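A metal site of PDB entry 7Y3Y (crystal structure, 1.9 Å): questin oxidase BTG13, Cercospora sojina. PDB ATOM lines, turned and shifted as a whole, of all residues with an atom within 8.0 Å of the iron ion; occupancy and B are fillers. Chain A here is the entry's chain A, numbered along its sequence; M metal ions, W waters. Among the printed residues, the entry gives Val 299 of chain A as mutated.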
ATOM      1  N   ALA A  51     -18.455  12.020 -38.775  1.00  0.00           N
ATOM      2  CA  ALA A  51     -19.083  12.740 -37.646  1.00  0.00           C
ATOM      3  C   ALA A  51     -20.542  13.072 -38.010  1.00  0.00           C
ATOM      4  O   ALA A  51     -21.016  14.206 -37.727  1.00  0.00           O
ATOM      5  CB  ALA A  51     -18.288  13.975 -37.329  1.00  0.00           C
ATOM      6  N   HIS A  53     -23.555  11.313 -37.322  1.00  0.00           N
ATOM      7  CA  HIS A  53     -24.534  10.433 -36.656  1.00  0.00           C
ATOM      8  C   HIS A  53     -25.773  11.261 -36.308  1.00  0.00           C
ATOM      9  O   HIS A  53     -25.614  12.427 -35.814  1.00  0.00           O
ATOM     10  CB  HIS A  53     -23.918   9.748 -35.429  1.00  0.00           C
ATOM     11  CG  HIS A  53     -22.561   9.162 -35.632  1.00  0.00           C
ATOM     12  ND1 HIS A  53     -21.399   9.904 -35.468  1.00  0.00           N
ATOM     13  CD2 HIS A  53     -22.159   7.892 -35.893  1.00  0.00           C
ATOM     14  CE1 HIS A  53     -20.360   9.133 -35.635  1.00  0.00           C
ATOM     15  NE2 HIS A  53     -20.794   7.877 -35.894  1.00  0.00           N
ATOM     16  N   ASN A  54     -26.959  10.714 -36.557  1.00  0.00           N
ATOM     17  CA  ASN A  54     -28.267  11.339 -36.202  1.00  0.00           C
ATOM     18  C   ASN A  54     -28.467  11.190 -34.671  1.00  0.00           C
ATOM     19  O   ASN A  54     -28.594  10.014 -34.193  1.00  0.00           O
ATOM     20  CB  ASN A  54     -29.391  10.682 -36.977  1.00  0.00           C
ATOM     21  CG  ASN A  54     -30.762  11.253 -36.628  1.00  0.00           C
ATOM     22  OD1 ASN A  54     -30.879  12.199 -35.826  1.00  0.00           O
ATOM     23  ND2 ASN A  54     -31.776  10.671 -37.242  1.00  0.00           N
ATOM     24  N   HIS A  55     -28.404  12.281 -33.921  1.00  0.00           N
ATOM     25  CA  HIS A  55     -28.516  12.253 -32.453  1.00  0.00           C
ATOM     26  C   HIS A  55     -29.965  12.468 -31.999  1.00  0.00           C
ATOM     27  O   HIS A  55     -30.188  12.498 -30.772  1.00  0.00           O
ATOM     28  CB  HIS A  55     -27.603  13.324 -31.825  1.00  0.00           C
ATOM     29  CG  HIS A  55     -26.143  12.987 -31.898  1.00  0.00           C
ATOM     30  ND1 HIS A  55     -25.502  12.808 -33.094  1.00  0.00           N
ATOM     31  CD2 HIS A  55     -25.225  12.809 -30.929  1.00  0.00           C
ATOM     32  CE1 HIS A  55     -24.248  12.516 -32.854  1.00  0.00           C
ATOM     33  NE2 HIS A  55     -24.045  12.519 -31.538  1.00  0.00           N
ATOM     34  N   HIS A  58     -31.321  10.297 -29.294  1.00  0.00           N
ATOM     35  CA  HIS A  58     -30.566  10.515 -28.045  1.00  0.00           C
ATOM     36  C   HIS A  58     -31.089  11.783 -27.327  1.00  0.00           C
ATOM     37  O   HIS A  58     -31.210  11.802 -26.075  1.00  0.00           O
ATOM     38  CB  HIS A  58     -29.066  10.672 -28.298  1.00  0.00           C
ATOM     39  CG  HIS A  58     -28.444   9.719 -29.278  1.00  0.00           C
ATOM     40  ND1 HIS A  58     -27.139   9.893 -29.687  1.00  0.00           N
ATOM     41  CD2 HIS A  58     -28.921   8.642 -29.957  1.00  0.00           C
ATOM     42  CE1 HIS A  58     -26.862   8.990 -30.616  1.00  0.00           C
ATOM     43  NE2 HIS A  58     -27.945   8.207 -30.801  1.00  0.00           N
ATOM     44  N   HIS A  83     -29.314  17.136 -38.253  1.00  0.00           N
ATOM     45  CA  HIS A  83     -29.034  15.684 -38.174  1.00  0.00           C
ATOM     46  C   HIS A  83     -30.036  14.901 -39.026  1.00  0.00           C
ATOM     47  O   HIS A  83     -29.865  13.699 -39.135  1.00  0.00           O
ATOM     48  CB  HIS A  83     -29.041  15.202 -36.725  1.00  0.00           C
ATOM     49  CG  HIS A  83     -27.892  15.679 -35.883  1.00  0.00           C
ATOM     50  ND1 HIS A  83     -27.520  15.030 -34.730  1.00  0.00           N
ATOM     51  CD2 HIS A  83     -27.118  16.790 -35.953  1.00  0.00           C
ATOM     52  CE1 HIS A  83     -26.505  15.682 -34.186  1.00  0.00           C
ATOM     53  NE2 HIS A  83     -26.267  16.787 -34.901  1.00  0.00           N
ATOM     54  N   GLY A 155     -17.053   5.207 -34.272  1.00  0.00           N
ATOM     55  CA  GLY A 155     -17.360   6.649 -34.321  1.00  0.00           C
ATOM     56  C   GLY A 155     -17.469   7.301 -32.943  1.00  0.00           C
ATOM     57  O   GLY A 155     -18.356   8.147 -32.795  1.00  0.00           O
ATOM     58  N   ALA A 156     -16.668   6.880 -31.983  1.00  0.00           N
ATOM     59  CA  ALA A 156     -16.682   7.384 -30.586  1.00  0.00           C
ATOM     60  C   ALA A 156     -18.032   6.983 -29.922  1.00  0.00           C
ATOM     61  O   ALA A 156     -18.689   7.826 -29.253  1.00  0.00           O
ATOM     62  CB  ALA A 156     -16.437   8.891 -30.618  1.00  0.00           C
ATOM     63  N   TYR A 157     -18.432   5.721 -30.100  1.00  0.00           N
ATOM     64  CA  TYR A 157     -19.461   4.991 -29.310  1.00  0.00           C
ATOM     65  C   TYR A 157     -20.885   5.265 -29.786  1.00  0.00           C
ATOM     66  O   TYR A 157     -21.795   4.868 -29.045  1.00  0.00           O
ATOM     67  CB  TYR A 157     -19.257   5.268 -27.806  1.00  0.00           C
ATOM     68  CG  TYR A 157     -17.850   5.026 -27.329  1.00  0.00           C
ATOM     69  CD1 TYR A 157     -17.306   3.759 -27.386  1.00  0.00           C
ATOM     70  CD2 TYR A 157     -17.052   6.053 -26.853  1.00  0.00           C
ATOM     71  CE1 TYR A 157     -16.026   3.509 -26.960  1.00  0.00           C
ATOM     72  CE2 TYR A 157     -15.764   5.829 -26.438  1.00  0.00           C
ATOM     73  CZ  TYR A 157     -15.234   4.546 -26.500  1.00  0.00           C
ATOM     74  OH  TYR A 157     -13.937   4.276 -26.142  1.00  0.00           O
ATOM     75  N   HIS A 158     -21.144   5.742 -31.014  1.00  0.00           N
ATOM     76  CA  HIS A 158     -22.536   6.072 -31.420  1.00  0.00           C
ATOM     77  C   HIS A 158     -23.427   4.825 -31.593  1.00  0.00           C
ATOM     78  O   HIS A 158     -24.578   4.853 -31.153  1.00  0.00           O
ATOM     79  CB  HIS A 158     -22.590   7.079 -32.567  1.00  0.00           C
ATOM     80  CG  HIS A 158     -22.159   8.447 -32.141  1.00  0.00           C
ATOM     81  ND1 HIS A 158     -20.844   8.892 -32.268  1.00  0.00           N
ATOM     82  CD2 HIS A 158     -22.854   9.476 -31.642  1.00  0.00           C
ATOM     83  CE1 HIS A 158     -20.794  10.134 -31.868  1.00  0.00           C
ATOM     84  NE2 HIS A 158     -22.010  10.502 -31.445  1.00  0.00           N
ATOM     85  N   ILE A 161     -24.351   3.738 -28.161  1.00  0.00           N
ATOM     86  CA  ILE A 161     -25.329   4.706 -27.604  1.00  0.00           C
ATOM     87  C   ILE A 161     -26.717   4.425 -28.204  1.00  0.00           C
ATOM     88  O   ILE A 161     -27.685   4.321 -27.437  1.00  0.00           O
ATOM     89  CB  ILE A 161     -24.819   6.143 -27.814  1.00  0.00           C
ATOM     90  CG1 ILE A 161     -23.589   6.440 -26.953  1.00  0.00           C
ATOM     91  CG2 ILE A 161     -25.943   7.127 -27.520  1.00  0.00           C
ATOM     92  CD1 ILE A 161     -22.783   7.642 -27.391  1.00  0.00           C
ATOM     93  N   PHE A 292     -14.448  17.130 -26.763  1.00  0.00           N
ATOM     94  CA  PHE A 292     -15.613  16.536 -27.470  1.00  0.00           C
ATOM     95  C   PHE A 292     -15.566  15.013 -27.360  1.00  0.00           C
ATOM     96  O   PHE A 292     -16.614  14.399 -27.100  1.00  0.00           O
ATOM     97  CB  PHE A 292     -15.611  17.009 -28.910  1.00  0.00           C
ATOM     98  CG  PHE A 292     -16.748  16.565 -29.787  1.00  0.00           C
ATOM     99  CD1 PHE A 292     -17.996  17.149 -29.669  1.00  0.00           C
ATOM    100  CD2 PHE A 292     -16.566  15.599 -30.764  1.00  0.00           C
ATOM    101  CE1 PHE A 292     -19.034  16.761 -30.504  1.00  0.00           C
ATOM    102  CE2 PHE A 292     -17.619  15.199 -31.576  1.00  0.00           C
ATOM    103  CZ  PHE A 292     -18.835  15.809 -31.454  1.00  0.00           C
ATOM    104  N   MET A 295     -15.886  13.730 -23.793  1.00  0.00           N
ATOM    105  CA  MET A 295     -17.338  13.823 -23.497  1.00  0.00           C
ATOM    106  C   MET A 295     -18.066  12.544 -23.993  1.00  0.00           C
ATOM    107  O   MET A 295     -18.892  11.966 -23.198  1.00  0.00           O
ATOM    108  CB  MET A 295     -17.894  15.113 -24.090  1.00  0.00           C
ATOM    109  CG  MET A 295     -19.403  15.242 -23.959  1.00  0.00           C
ATOM    110  SD  MET A 295     -20.211  14.565 -25.473  1.00  0.00           S
ATOM    111  CE  MET A 295     -19.745  15.809 -26.648  1.00  0.00           C
ATOM    112  N   HIS A 296     -17.729  12.046 -25.200  1.00  0.00           N
ATOM    113  CA  HIS A 296     -18.290  10.785 -25.768  1.00  0.00           C
ATOM    114  C   HIS A 296     -17.872   9.597 -24.908  1.00  0.00           C
ATOM    115  O   HIS A 296     -18.729   8.748 -24.634  1.00  0.00           O
ATOM    116  CB  HIS A 296     -17.897  10.614 -27.263  1.00  0.00           C
ATOM    117  CG  HIS A 296     -18.792  11.398 -28.151  1.00  0.00           C
ATOM    118  ND1 HIS A 296     -18.627  12.756 -28.338  1.00  0.00           N
ATOM    119  CD2 HIS A 296     -19.923  11.037 -28.820  1.00  0.00           C
ATOM    120  CE1 HIS A 296     -19.586  13.196 -29.145  1.00  0.00           C
ATOM    121  NE2 HIS A 296     -20.417  12.150 -29.446  1.00  0.00           N
ATOM    122  N   VAL A 299     -20.313  10.001 -21.916  1.00  0.00           N
ATOM    123  CA  VAL A 299     -21.750   9.771 -22.216  1.00  0.00           C
ATOM    124  C   VAL A 299     -21.993   8.281 -22.460  1.00  0.00           C
ATOM    125  O   VAL A 299     -23.056   7.822 -22.027  1.00  0.00           O
ATOM    126  CB  VAL A 299     -22.399  10.616 -23.321  1.00  0.00           C
ATOM    127  CG1 VAL A 299     -21.983  12.085 -23.337  1.00  0.00           C
ATOM    128  CG2 VAL A 299     -22.357   9.966 -24.657  1.00  0.00           C
ATOM    129  N   ASP A 372     -27.508  19.863 -29.268  1.00  0.00           N
ATOM    130  CA  ASP A 372     -27.776  18.689 -30.142  1.00  0.00           C
ATOM    131  C   ASP A 372     -28.008  17.424 -29.327  1.00  0.00           C
ATOM    132  O   ASP A 372     -28.309  16.410 -29.942  1.00  0.00           O
ATOM    133  CB  ASP A 372     -26.621  18.412 -31.091  1.00  0.00           C
ATOM    134  CG  ASP A 372     -25.234  18.347 -30.488  1.00  0.00           C
ATOM    135  OD1 ASP A 372     -25.073  18.308 -29.266  1.00  0.00           O
ATOM    136  OD2 ASP A 372     -24.338  18.327 -31.299  1.00  0.00           O
ATOM    137  N   GLY A 373     -27.932  17.513 -27.992  1.00  0.00           N
ATOM    138  CA  GLY A 373     -28.188  16.364 -27.097  1.00  0.00           C
ATOM    139  C   GLY A 373     -26.986  15.989 -26.254  1.00  0.00           C
ATOM    140  O   GLY A 373     -27.184  15.315 -25.198  1.00  0.00           O
ATOM    141  N   HIS A 374     -25.764  16.424 -26.595  1.00  0.00           N
ATOM    142  CA  HIS A 374     -24.576  15.960 -25.824  1.00  0.00           C
ATOM    143  C   HIS A 374     -24.653  16.503 -24.377  1.00  0.00           C
ATOM    144  O   HIS A 374     -24.181  15.800 -23.472  1.00  0.00           O
ATOM    145  CB  HIS A 374     -23.268  16.330 -26.526  1.00  0.00           C
ATOM    146  CG  HIS A 374     -23.069  15.613 -27.819  1.00  0.00           C
ATOM    147  ND1 HIS A 374     -23.354  16.202 -29.032  1.00  0.00           N
ATOM    148  CD2 HIS A 374     -22.649  14.352 -28.080  1.00  0.00           C
ATOM    149  CE1 HIS A 374     -23.097  15.328 -30.009  1.00  0.00           C
ATOM    150  NE2 HIS A 374     -22.629  14.188 -29.451  1.00  0.00           N
ATOM    151  N   LYS A 377     -26.933  14.353 -22.398  1.00  0.00           N
ATOM    152  CA  LYS A 377     -26.301  13.004 -22.232  1.00  0.00           C
ATOM    153  C   LYS A 377     -25.162  13.038 -21.204  1.00  0.00           C
ATOM    154  O   LYS A 377     -25.139  12.101 -20.350  1.00  0.00           O
ATOM    155  CB  LYS A 377     -25.755  12.504 -23.566  1.00  0.00           C
ATOM    156  CG  LYS A 377     -26.912  11.927 -24.341  1.00  0.00           C
ATOM    157  CD  LYS A 377     -26.764  11.830 -25.787  1.00  0.00           C
ATOM    158  CE  LYS A 377     -25.472  11.220 -26.237  1.00  0.00           C
ATOM    159  NZ  LYS A 377     -25.344  11.468 -27.679  1.00  0.00           N
HETATM  160 FE    FE M   1     -22.239  12.361 -30.411  1.00  0.00          FE
HETATM  161  O   HOH W   1     -23.153  11.204 -28.797  1.00  0.00           O
HETATM  162  O   HOH W   2     -21.238  13.412 -31.975  1.00  0.00           O
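The iron ion is bound by NE2 of His 296 (2.1 Å), NE2 of His 374 (2.1 Å), water W2 (2.1 Å), NE2 of His 55 (2.1 Å), NE2 of His 158 (2.1 Å) and water W1 (2.2 Å). The iron ion has six donor atoms within binding distance.
Within 4 Å of the iron ion: His 55, His 158, His 296 and His 374.
A ring nitrogen (ND1) of His 158 is in hydrogen-bond range of a ring nitrogen (ND1) of His 53, 3.4 Å away. A ring nitrogen (ND1) of His 158 sits at hydrogen-bond distance from the backbone carbonyl oxygen (O) of Gly 155, 2.7 Å away. The backbone carbonyl oxygen (O) of Phe 292 sits at hydrogen-bond distance from a ring nitrogen (ND1) of His 296, at 2.9 Å. OD1 of Asp 372 lies within hydrogen-bond range of ND1 of His 374. ND1 of His 296 lies close to SD of Met 295. ND1 of His 55 lies within hydrogen-bond range of O of His 53 (2.7 Å). The backbone NH (N) of His 55 is in hydrogen-bond range of a ring nitrogen (ND1) of His 83.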
